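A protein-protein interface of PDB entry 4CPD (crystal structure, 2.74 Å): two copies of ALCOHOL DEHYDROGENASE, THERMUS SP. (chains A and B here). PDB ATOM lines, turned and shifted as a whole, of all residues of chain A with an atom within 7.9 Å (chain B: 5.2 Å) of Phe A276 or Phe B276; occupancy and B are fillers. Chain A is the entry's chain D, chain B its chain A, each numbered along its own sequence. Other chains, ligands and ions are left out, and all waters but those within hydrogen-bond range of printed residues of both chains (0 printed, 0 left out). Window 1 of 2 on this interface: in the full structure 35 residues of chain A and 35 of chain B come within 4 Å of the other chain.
The backbone carbonyl oxygen of Pro B272 is in hydrogen-bond range of the backbone NH of Leu A278 (3.0 Å).
The backbone NH (N) of Phe A276 lies within hydrogen-bond range of the backbone carbonyl oxygen (O) of Phe B274, 2.9 Å away.
The backbone carbonyl oxygen of Phe A274 is in hydrogen-bond range of the backbone NH of Phe B276 (2.8 Å).
The backbone carbonyl oxygen of Pro A272 lies within hydrogen-bond range of the backbone NH of Leu B278 (3.0 Å).
N of Leu B286 is in hydrogen-bond range of O of Ile A290 (3.1 Å).
The backbone carbonyl oxygen of Phe B288 lies within hydrogen-bond range of the backbone NH of Phe A288 (2.8 Å).
The backbone carbonyl oxygen (O) of Leu A286 sits at hydrogen-bond distance from the backbone NH (N) of Ile B290 (3.2 Å).
O of Phe A274 lies close to O of Phe B274, at 3.5 Å.
N of Val A263 lies within hydrogen-bond range of O of Thr A287, at 2.8 Å.
The backbone carbonyl oxygen (O) of Val A263 is in hydrogen-bond range of the backbone NH (N) of Arg A289 (3.0 Å).
Leu B278 touches Leu A250.
Ala A271 touches Leu B278 (O to CB, 3.4 Å).
Pro A272 touches Pro B277 (O to CA, 3.5 Å).
O of Phe B276 touches CA of Ser A273, 3.2 Å away.
Ser B273 touches Pro A275 (OG to CB, 3.8 Å).
Ser B273 touches Phe A276 (CA to O, 3.2 Å).
Phe A276 touches Phe B276.
Phe A276 touches Ile B290 (CE1 to CG2, 3.99 Å).
Leu A282 touches Ile B290.
Arg A289 touches Leu B286.
Of the printed residues of chain A, Phe B276 touches Ser A273 (3.2 Å), Phe A274 (2.8 Å), Phe A276 (3.8 Å) and Phe A288 (3.9 Å).
Pro B277 touches just one residue of chain A: Pro A272 (3.5 Å).
Of the printed residues of chain B, Leu A250 touches Leu B278 (3.8 Å).
Of the printed residues of chain B, Arg A289 touches Leu B286.
Of the printed residues of chain B, Pro A272 touches Pro B277 (3.5 Å) and Leu B278 (3.0 Å).
The nearest printed residue of chain A that does not touch Phe B276 is Ile A290 (4.001 Å).
The nearest printed residue of chain A that does not touch Ile B290 is Leu A278 (4.2 Å).
Printed residues of chain A that touch a printed residue of chain B: Leu A250, Ala A271, Pro A272, Ser A273, Phe A274, Pro A275, Phe A276, Pro A277, Leu A278, Gly A281, Leu A282, Asp A285, Leu A286, Thr A287, Phe A288, Arg A289 and Ile A290.
Hydrophobic or aromatic side chains of chain A within 4 Å of the printed part of chain B: Leu A250, Phe A274, Pro A275, Phe A276, Leu A278, Leu A282 and Phe A288.
Hydrophobic or aromatic side chains of chain B within 4 Å of the printed part of chain A: Phe B274, Pro B275, Phe B276, Leu B278, Phe B288 and Ile B290.
Among the printed residues, 32 pairs touch across the chains.
Pro A272 touches Leu B278, and with the chains exchanged Leu A278 touches Pro B272.
Phe A274 touches Phe B276, and with the chains exchanged Phe A276 touches Phe B274.
Leu A278 touches Phe B274, but with the chains exchanged Phe A274 does not touch Leu B278 (4.1 Å).
Leu A286 touches Phe B288, and with the chains exchanged Phe A288 touches Leu B286.
11 positions are printed for both chains.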
ATOM      1  N   LEU A 250     -10.962 -33.128  14.863  1.00  0.00           N
ATOM      2  CA  LEU A 250     -11.821 -32.011  14.428  1.00  0.00           C
ATOM      3  C   LEU A 250     -11.099 -31.137  13.437  1.00  0.00           C
ATOM      4  O   LEU A 250     -11.679 -30.736  12.423  1.00  0.00           O
ATOM      5  CB  LEU A 250     -12.349 -31.179  15.610  1.00  0.00           C
ATOM      6  CG  LEU A 250     -13.384 -31.951  16.456  1.00  0.00           C
ATOM      7  CD1 LEU A 250     -13.564 -31.376  17.864  1.00  0.00           C
ATOM      8  CD2 LEU A 250     -14.713 -32.043  15.721  1.00  0.00           C
ATOM      9  N   SER A 251      -9.833 -30.847  13.706  1.00  0.00           N
ATOM     10  CA  SER A 251      -9.064 -30.001  12.792  1.00  0.00           C
ATOM     11  C   SER A 251      -8.894 -30.744  11.491  1.00  0.00           C
ATOM     12  O   SER A 251      -8.964 -30.170  10.408  1.00  0.00           O
ATOM     13  CB  SER A 251      -7.723 -29.625  13.403  1.00  0.00           C
ATOM     14  OG  SER A 251      -7.973 -29.156  14.724  1.00  0.00           O
ATOM     15  N   LEU A 254     -12.010 -30.463   9.431  1.00  0.00           N
ATOM     16  CA  LEU A 254     -12.191 -29.151   8.848  1.00  0.00           C
ATOM     17  C   LEU A 254     -11.235 -28.874   7.720  1.00  0.00           C
ATOM     18  O   LEU A 254     -11.546 -28.080   6.837  1.00  0.00           O
ATOM     19  CB  LEU A 254     -12.111 -28.063   9.920  1.00  0.00           C
ATOM     20  CG  LEU A 254     -13.322 -28.087  10.861  1.00  0.00           C
ATOM     21  CD1 LEU A 254     -13.062 -27.373  12.177  1.00  0.00           C
ATOM     22  CD2 LEU A 254     -14.497 -27.459  10.158  1.00  0.00           C
ATOM     23  N   VAL A 263     -19.491 -30.229   8.100  1.00  0.00           N
ATOM     24  CA  VAL A 263     -18.869 -31.130   9.060  1.00  0.00           C
ATOM     25  C   VAL A 263     -19.858 -31.370  10.177  1.00  0.00           C
ATOM     26  O   VAL A 263     -20.420 -30.432  10.750  1.00  0.00           O
ATOM     27  CB  VAL A 263     -17.536 -30.574   9.615  1.00  0.00           C
ATOM     28  CG1 VAL A 263     -16.988 -31.461  10.714  1.00  0.00           C
ATOM     29  CG2 VAL A 263     -16.483 -30.459   8.507  1.00  0.00           C
ATOM     30  N   ALA A 271     -11.819 -31.670  26.462  1.00  0.00           N
ATOM     31  CA  ALA A 271     -11.061 -30.431  26.261  1.00  0.00           C
ATOM     32  C   ALA A 271     -12.087 -29.318  26.237  1.00  0.00           C
ATOM     33  O   ALA A 271     -13.185 -29.526  25.729  1.00  0.00           O
ATOM     34  CB  ALA A 271     -10.263 -30.486  24.952  1.00  0.00           C
ATOM     35  N   PRO A 272     -11.767 -28.145  26.812  1.00  0.00           N
ATOM     36  CA  PRO A 272     -12.752 -27.057  26.747  1.00  0.00           C
ATOM     37  C   PRO A 272     -12.889 -26.412  25.349  1.00  0.00           C
ATOM     38  O   PRO A 272     -13.912 -25.805  25.069  1.00  0.00           O
ATOM     39  CB  PRO A 272     -12.199 -26.041  27.750  1.00  0.00           C
ATOM     40  CG  PRO A 272     -10.726 -26.203  27.652  1.00  0.00           C
ATOM     41  CD  PRO A 272     -10.465 -27.656  27.304  1.00  0.00           C
ATOM     42  N   SER A 273     -11.880 -26.557  24.481  1.00  0.00           N
ATOM     43  CA  SER A 273     -11.889 -25.884  23.186  1.00  0.00           C
ATOM     44  C   SER A 273     -10.971 -26.517  22.113  1.00  0.00           C
ATOM     45  O   SER A 273     -10.190 -27.431  22.405  1.00  0.00           O
ATOM     46  CB  SER A 273     -11.487 -24.426  23.379  1.00  0.00           C
ATOM     47  OG  SER A 273     -10.130 -24.260  23.039  1.00  0.00           O
ATOM     48  N   PHE A 274     -11.105 -26.018  20.875  1.00  0.00           N
ATOM     49  CA  PHE A 274     -10.205 -26.349  19.761  1.00  0.00           C
ATOM     50  C   PHE A 274     -10.104 -25.179  18.772  1.00  0.00           C
ATOM     51  O   PHE A 274     -11.015 -24.370  18.675  1.00  0.00           O
ATOM     52  CB  PHE A 274     -10.658 -27.626  19.053  1.00  0.00           C
ATOM     53  CG  PHE A 274     -11.847 -27.449  18.145  1.00  0.00           C
ATOM     54  CD1 PHE A 274     -13.140 -27.566  18.640  1.00  0.00           C
ATOM     55  CD2 PHE A 274     -11.678 -27.207  16.790  1.00  0.00           C
ATOM     56  CE1 PHE A 274     -14.237 -27.409  17.801  1.00  0.00           C
ATOM     57  CE2 PHE A 274     -12.769 -27.047  15.949  1.00  0.00           C
ATOM     58  CZ  PHE A 274     -14.048 -27.146  16.455  1.00  0.00           C
ATOM     59  N   PRO A 275      -8.988 -25.072  18.038  1.00  0.00           N
ATOM     60  CA  PRO A 275      -8.852 -23.936  17.119  1.00  0.00           C
ATOM     61  C   PRO A 275      -9.626 -24.116  15.795  1.00  0.00           C
ATOM     62  O   PRO A 275      -9.304 -24.986  14.985  1.00  0.00           O
ATOM     63  CB  PRO A 275      -7.346 -23.884  16.865  1.00  0.00           C
ATOM     64  CG  PRO A 275      -6.930 -25.322  16.964  1.00  0.00           C
ATOM     65  CD  PRO A 275      -7.832 -25.983  17.964  1.00  0.00           C
ATOM     66  N   PHE A 276     -10.634 -23.276  15.597  1.00  0.00           N
ATOM     67  CA  PHE A 276     -11.439 -23.290  14.387  1.00  0.00           C
ATOM     68  C   PHE A 276     -10.829 -22.296  13.433  1.00  0.00           C
ATOM     69  O   PHE A 276     -10.579 -21.157  13.817  1.00  0.00           O
ATOM     70  CB  PHE A 276     -12.875 -22.871  14.707  1.00  0.00           C
ATOM     71  CG  PHE A 276     -13.861 -23.242  13.646  1.00  0.00           C
ATOM     72  CD1 PHE A 276     -13.946 -22.499  12.475  1.00  0.00           C
ATOM     73  CD2 PHE A 276     -14.716 -24.316  13.823  1.00  0.00           C
ATOM     74  CE1 PHE A 276     -14.837 -22.831  11.480  1.00  0.00           C
ATOM     75  CE2 PHE A 276     -15.618 -24.663  12.832  1.00  0.00           C
ATOM     76  CZ  PHE A 276     -15.673 -23.922  11.658  1.00  0.00           C
ATOM     77  N   PRO A 277     -10.604 -22.702  12.182  1.00  0.00           N
ATOM     78  CA  PRO A 277     -10.058 -21.773  11.204  1.00  0.00           C
ATOM     79  C   PRO A 277     -10.922 -20.578  10.958  1.00  0.00           C
ATOM     80  O   PRO A 277     -12.097 -20.741  10.693  1.00  0.00           O
ATOM     81  CB  PRO A 277     -10.009 -22.586   9.909  1.00  0.00           C
ATOM     82  CG  PRO A 277     -10.850 -23.767  10.142  1.00  0.00           C
ATOM     83  CD  PRO A 277     -10.808 -24.036  11.616  1.00  0.00           C
ATOM     84  N   LEU A 278     -10.314 -19.398  10.995  1.00  0.00           N
ATOM     85  CA  LEU A 278     -11.028 -18.139  10.822  1.00  0.00           C
ATOM     86  C   LEU A 278     -10.809 -17.582   9.422  1.00  0.00           C
ATOM     87  O   LEU A 278     -11.716 -17.690   8.579  1.00  0.00           O
ATOM     88  CB  LEU A 278     -10.622 -17.149  11.903  1.00  0.00           C
ATOM     89  CG  LEU A 278     -11.665 -16.121  12.277  1.00  0.00           C
ATOM     90  CD1 LEU A 278     -11.262 -15.440  13.570  1.00  0.00           C
ATOM     91  CD2 LEU A 278     -11.822 -15.103  11.164  1.00  0.00           C
ATOM     92  N   ALA A 279      -9.624 -17.031   9.154  1.00  0.00           N
ATOM     93  CA  ALA A 279      -9.342 -16.418   7.845  1.00  0.00           C
ATOM     94  C   ALA A 279      -9.538 -17.416   6.724  1.00  0.00           C
ATOM     95  O   ALA A 279     -10.218 -17.137   5.721  1.00  0.00           O
ATOM     96  CB  ALA A 279      -7.940 -15.861   7.808  1.00  0.00           C
ATOM     97  N   SER A 280      -8.963 -18.596   6.917  1.00  0.00           N
ATOM     98  CA  SER A 280      -9.168 -19.692   5.961  1.00  0.00           C
ATOM     99  C   SER A 280     -10.617 -20.213   5.991  1.00  0.00           C
ATOM    100  O   SER A 280     -11.129 -20.690   4.978  1.00  0.00           O
ATOM    101  CB  SER A 280      -8.167 -20.829   6.190  1.00  0.00           C
ATOM    102  OG  SER A 280      -8.517 -21.589   7.318  1.00  0.00           O
ATOM    103  N   GLY A 281     -11.257 -20.125   7.155  1.00  0.00           N
ATOM    104  CA  GLY A 281     -12.660 -20.510   7.296  1.00  0.00           C
ATOM    105  C   GLY A 281     -13.588 -19.673   6.447  1.00  0.00           C
ATOM    106  O   GLY A 281     -14.491 -20.214   5.789  1.00  0.00           O
ATOM    107  N   LEU A 282     -13.355 -18.363   6.459  1.00  0.00           N
ATOM    108  CA  LEU A 282     -14.118 -17.450   5.640  1.00  0.00           C
ATOM    109  C   LEU A 282     -14.000 -17.789   4.174  1.00  0.00           C
ATOM    110  O   LEU A 282     -14.999 -17.788   3.453  1.00  0.00           O
ATOM    111  CB  LEU A 282     -13.634 -16.024   5.840  1.00  0.00           C
ATOM    112  CG  LEU A 282     -14.041 -15.364   7.157  1.00  0.00           C
ATOM    113  CD1 LEU A 282     -13.180 -14.130   7.413  1.00  0.00           C
ATOM    114  CD2 LEU A 282     -15.527 -15.002   7.107  1.00  0.00           C
ATOM    115  N   ASP A 285     -15.901 -21.263   3.444  1.00  0.00           N
ATOM    116  CA  ASP A 285     -17.339 -21.397   3.606  1.00  0.00           C
ATOM    117  C   ASP A 285     -17.689 -22.742   4.277  1.00  0.00           C
ATOM    118  O   ASP A 285     -18.197 -23.665   3.670  1.00  0.00           O
ATOM    119  CB  ASP A 285     -18.071 -21.238   2.256  1.00  0.00           C
ATOM    120  CG  ASP A 285     -19.545 -20.910   2.418  1.00  0.00           C
ATOM    121  OD1 ASP A 285     -20.033 -20.934   3.571  1.00  0.00           O
ATOM    122  OD2 ASP A 285     -20.212 -20.629   1.390  1.00  0.00           O
ATOM    123  N   LEU A 286     -17.419 -22.822   5.561  1.00  0.00           N
ATOM    124  CA  LEU A 286     -17.689 -24.019   6.308  1.00  0.00           C
ATOM    125  C   LEU A 286     -19.006 -23.965   7.096  1.00  0.00           C
ATOM    126  O   LEU A 286     -19.350 -22.937   7.693  1.00  0.00           O
ATOM    127  CB  LEU A 286     -16.538 -24.212   7.301  1.00  0.00           C
ATOM    128  CG  LEU A 286     -15.168 -24.443   6.672  1.00  0.00           C
ATOM    129  CD1 LEU A 286     -14.088 -24.257   7.716  1.00  0.00           C
ATOM    130  CD2 LEU A 286     -15.095 -25.832   6.038  1.00  0.00           C
ATOM    131  N   THR A 287     -19.706 -25.090   7.134  1.00  0.00           N
ATOM    132  CA  THR A 287     -20.792 -25.290   8.074  1.00  0.00           C
ATOM    133  C   THR A 287     -20.397 -26.388   9.050  1.00  0.00           C
ATOM    134  O   THR A 287     -20.083 -27.496   8.649  1.00  0.00           O
ATOM    135  CB  THR A 287     -22.061 -25.703   7.314  1.00  0.00           C
ATOM    136  OG1 THR A 287     -22.391 -24.671   6.369  1.00  0.00           O
ATOM    137  CG2 THR A 287     -23.241 -25.941   8.269  1.00  0.00           C
ATOM    138  N   PHE A 288     -20.460 -26.094  10.332  1.00  0.00           N
ATOM    139  CA  PHE A 288     -20.026 -27.024  11.388  1.00  0.00           C
ATOM    140  C   PHE A 288     -21.090 -27.262  12.449  1.00  0.00           C
ATOM    141  O   PHE A 288     -21.759 -26.355  12.877  1.00  0.00           O
ATOM    142  CB  PHE A 288     -18.779 -26.448  12.056  1.00  0.00           C
ATOM    143  CG  PHE A 288     -18.235 -27.290  13.165  1.00  0.00           C
ATOM    144  CD1 PHE A 288     -17.563 -28.445  12.897  1.00  0.00           C
ATOM    145  CD2 PHE A 288     -18.412 -26.928  14.480  1.00  0.00           C
ATOM    146  CE1 PHE A 288     -17.088 -29.239  13.925  1.00  0.00           C
ATOM    147  CE2 PHE A 288     -17.931 -27.711  15.513  1.00  0.00           C
ATOM    148  CZ  PHE A 288     -17.270 -28.862  15.236  1.00  0.00           C
ATOM    149  N   ARG A 289     -21.271 -28.495  12.855  1.00  0.00           N
ATOM    150  CA  ARG A 289     -22.200 -28.789  13.932  1.00  0.00           C
ATOM    151  C   ARG A 289     -21.584 -29.787  14.866  1.00  0.00           C
ATOM    152  O   ARG A 289     -20.981 -30.753  14.443  1.00  0.00           O
ATOM    153  CB  ARG A 289     -23.544 -29.321  13.424  1.00  0.00           C
ATOM    154  CG  ARG A 289     -24.570 -29.384  14.565  1.00  0.00           C
ATOM    155  CD  ARG A 289     -25.994 -29.616  14.064  1.00  0.00           C
ATOM    156  NE  ARG A 289     -26.976 -29.711  15.151  1.00  0.00           N
ATOM    157  CZ  ARG A 289     -28.278 -29.925  14.966  1.00  0.00           C
ATOM    158  NH1 ARG A 289     -28.761 -30.039  13.730  1.00  0.00           N
ATOM    159  NH2 ARG A 289     -29.096 -30.010  16.007  1.00  0.00           N
ATOM    160  N   ILE A 290     -21.747 -29.532  16.150  1.00  0.00           N
ATOM    161  CA  ILE A 290     -21.251 -30.408  17.203  1.00  0.00           C
ATOM    162  C   ILE A 290     -22.326 -30.551  18.280  1.00  0.00           C
ATOM    163  O   ILE A 290     -22.973 -29.589  18.674  1.00  0.00           O
ATOM    164  CB  ILE A 290     -19.932 -29.888  17.784  1.00  0.00           C
ATOM    165  CG1 ILE A 290     -19.458 -30.803  18.891  1.00  0.00           C
ATOM    166  CG2 ILE A 290     -20.069 -28.477  18.316  1.00  0.00           C
ATOM    167  CD1 ILE A 290     -17.965 -30.686  19.115  1.00  0.00           C
ATOM    168  N   LEU B 254     -20.902 -17.239  20.242  1.00  0.00           N
ATOM    169  CA  LEU B 254     -21.038 -18.634  20.674  1.00  0.00           C
ATOM    170  C   LEU B 254     -21.457 -18.794  22.141  1.00  0.00           C
ATOM    171  O   LEU B 254     -22.161 -19.733  22.499  1.00  0.00           O
ATOM    172  CB  LEU B 254     -19.756 -19.406  20.377  1.00  0.00           C
ATOM    173  CG  LEU B 254     -19.579 -19.639  18.873  1.00  0.00           C
ATOM    174  CD1 LEU B 254     -18.159 -20.024  18.554  1.00  0.00           C
ATOM    175  CD2 LEU B 254     -20.519 -20.711  18.332  1.00  0.00           C
ATOM    176  N   PRO B 272      -5.720 -16.455  12.126  1.00  0.00           N
ATOM    177  CA  PRO B 272      -5.849 -17.734  11.438  1.00  0.00           C
ATOM    178  C   PRO B 272      -6.874 -18.636  12.120  1.00  0.00           C
ATOM    179  O   PRO B 272      -7.380 -19.566  11.499  1.00  0.00           O
ATOM    180  CB  PRO B 272      -4.435 -18.316  11.526  1.00  0.00           C
ATOM    181  CG  PRO B 272      -3.889 -17.743  12.800  1.00  0.00           C
ATOM    182  CD  PRO B 272      -4.531 -16.398  12.992  1.00  0.00           C
ATOM    183  N   SER B 273      -7.189 -18.351  13.379  1.00  0.00           N
ATOM    184  CA  SER B 273      -8.050 -19.228  14.157  1.00  0.00           C
ATOM    185  C   SER B 273      -8.697 -18.531  15.366  1.00  0.00           C
ATOM    186  O   SER B 273      -8.344 -17.407  15.729  1.00  0.00           O
ATOM    187  CB  SER B 273      -7.249 -20.443  14.642  1.00  0.00           C
ATOM    188  OG  SER B 273      -6.806 -20.228  15.983  1.00  0.00           O
ATOM    189  N   PHE B 274      -9.652 -19.229  15.978  1.00  0.00           N
ATOM    190  CA  PHE B 274     -10.250 -18.818  17.256  1.00  0.00           C
ATOM    191  C   PHE B 274     -10.702 -20.063  18.055  1.00  0.00           C
ATOM    192  O   PHE B 274     -10.999 -21.102  17.460  1.00  0.00           O
ATOM    193  CB  PHE B 274     -11.429 -17.853  17.009  1.00  0.00           C
ATOM    194  CG  PHE B 274     -12.678 -18.531  16.498  1.00  0.00           C
ATOM    195  CD1 PHE B 274     -12.885 -18.703  15.142  1.00  0.00           C
ATOM    196  CD2 PHE B 274     -13.638 -19.014  17.384  1.00  0.00           C
ATOM    197  CE1 PHE B 274     -14.022 -19.352  14.675  1.00  0.00           C
ATOM    198  CE2 PHE B 274     -14.773 -19.653  16.922  1.00  0.00           C
ATOM    199  CZ  PHE B 274     -14.966 -19.818  15.563  1.00  0.00           C
ATOM    200  N   PRO B 275     -10.775 -19.959  19.400  1.00  0.00           N
ATOM    201  CA  PRO B 275     -11.146 -21.133  20.212  1.00  0.00           C
ATOM    202  C   PRO B 275     -12.647 -21.461  20.192  1.00  0.00           C
ATOM    203  O   PRO B 275     -13.470 -20.696  20.710  1.00  0.00           O
ATOM    204  CB  PRO B 275     -10.708 -20.730  21.626  1.00  0.00           C
ATOM    205  CG  PRO B 275     -10.820 -19.234  21.647  1.00  0.00           C
ATOM    206  CD  PRO B 275     -10.590 -18.750  20.231  1.00  0.00           C
ATOM    207  N   PHE B 276     -12.994 -22.595  19.595  1.00  0.00           N
ATOM    208  CA  PHE B 276     -14.391 -23.032  19.503  1.00  0.00           C
ATOM    209  C   PHE B 276     -14.636 -23.965  20.656  1.00  0.00           C
ATOM    210  O   PHE B 276     -13.853 -24.887  20.830  1.00  0.00           O
ATOM    211  CB  PHE B 276     -14.643 -23.780  18.201  1.00  0.00           C
ATOM    212  CG  PHE B 276     -16.084 -23.909  17.855  1.00  0.00           C
ATOM    213  CD1 PHE B 276     -16.884 -24.808  18.519  1.00  0.00           C
ATOM    214  CD2 PHE B 276     -16.640 -23.133  16.859  1.00  0.00           C
ATOM    215  CE1 PHE B 276     -18.229 -24.926  18.222  1.00  0.00           C
ATOM    216  CE2 PHE B 276     -17.990 -23.239  16.549  1.00  0.00           C
ATOM    217  CZ  PHE B 276     -18.786 -24.138  17.226  1.00  0.00           C
ATOM    218  N   PRO B 277     -15.708 -23.733  21.448  1.00  0.00           N
ATOM    219  CA  PRO B 277     -15.984 -24.578  22.597  1.00  0.00           C
ATOM    220  C   PRO B 277     -16.245 -26.010  22.190  1.00  0.00           C
ATOM    221  O   PRO B 277     -17.021 -26.264  21.258  1.00  0.00           O
ATOM    222  CB  PRO B 277     -17.257 -23.978  23.197  1.00  0.00           C
ATOM    223  CG  PRO B 277     -17.826 -23.095  22.151  1.00  0.00           C
ATOM    224  CD  PRO B 277     -16.656 -22.610  21.365  1.00  0.00           C
ATOM    225  N   LEU B 278     -15.606 -26.932  22.905  1.00  0.00           N
ATOM    226  CA  LEU B 278     -15.682 -28.345  22.596  1.00  0.00           C
ATOM    227  C   LEU B 278     -16.610 -29.040  23.592  1.00  0.00           C
ATOM    228  O   LEU B 278     -17.727 -29.388  23.259  1.00  0.00           O
ATOM    229  CB  LEU B 278     -14.283 -28.954  22.564  1.00  0.00           C
ATOM    230  CG  LEU B 278     -14.119 -30.162  21.645  1.00  0.00           C
ATOM    231  CD1 LEU B 278     -12.645 -30.471  21.438  1.00  0.00           C
ATOM    232  CD2 LEU B 278     -14.852 -31.391  22.178  1.00  0.00           C
ATOM    233  N   LEU B 286     -24.348 -26.803  18.983  1.00  0.00           N
ATOM    234  CA  LEU B 286     -24.175 -25.574  18.224  1.00  0.00           C
ATOM    235  C   LEU B 286     -24.117 -25.871  16.743  1.00  0.00           C
ATOM    236  O   LEU B 286     -23.511 -26.861  16.345  1.00  0.00           O
ATOM    237  CB  LEU B 286     -22.896 -24.859  18.652  1.00  0.00           C
ATOM    238  CG  LEU B 286     -22.877 -24.326  20.098  1.00  0.00           C
ATOM    239  CD1 LEU B 286     -21.456 -24.027  20.546  1.00  0.00           C
ATOM    240  CD2 LEU B 286     -23.762 -23.093  20.252  1.00  0.00           C
ATOM    241  N   PHE B 288     -22.779 -23.773  13.439  1.00  0.00           N
ATOM    242  CA  PHE B 288     -21.952 -22.605  13.153  1.00  0.00           C
ATOM    243  C   PHE B 288     -21.640 -22.551  11.666  1.00  0.00           C
ATOM    244  O   PHE B 288     -21.318 -23.564  11.061  1.00  0.00           O
ATOM    245  CB  PHE B 288     -20.652 -22.664  13.955  1.00  0.00           C
ATOM    246  CG  PHE B 288     -19.708 -21.525  13.682  1.00  0.00           C
ATOM    247  CD1 PHE B 288     -19.915 -20.288  14.252  1.00  0.00           C
ATOM    248  CD2 PHE B 288     -18.585 -21.698  12.890  1.00  0.00           C
ATOM    249  CE1 PHE B 288     -19.032 -19.228  14.017  1.00  0.00           C
ATOM    250  CE2 PHE B 288     -17.699 -20.645  12.643  1.00  0.00           C
ATOM    251  CZ  PHE B 288     -17.916 -19.408  13.210  1.00  0.00           C
ATOM    252  N   ILE B 290     -19.510 -19.954   8.737  1.00  0.00           N
ATOM    253  CA  ILE B 290     -18.665 -18.792   8.456  1.00  0.00           C
ATOM    254  C   ILE B 290     -18.305 -18.792   6.984  1.00  0.00           C
ATOM    255  O   ILE B 290     -17.991 -19.829   6.423  1.00  0.00           O
ATOM    256  CB  ILE B 290     -17.390 -18.777   9.328  1.00  0.00           C
ATOM    257  CG1 ILE B 290     -16.509 -17.576   8.976  1.00  0.00           C
ATOM    258  CG2 ILE B 290     -16.587 -20.069   9.198  1.00  0.00           C
ATOM    259  CD1 ILE B 290     -15.600 -17.160  10.119  1.00  0.00           C
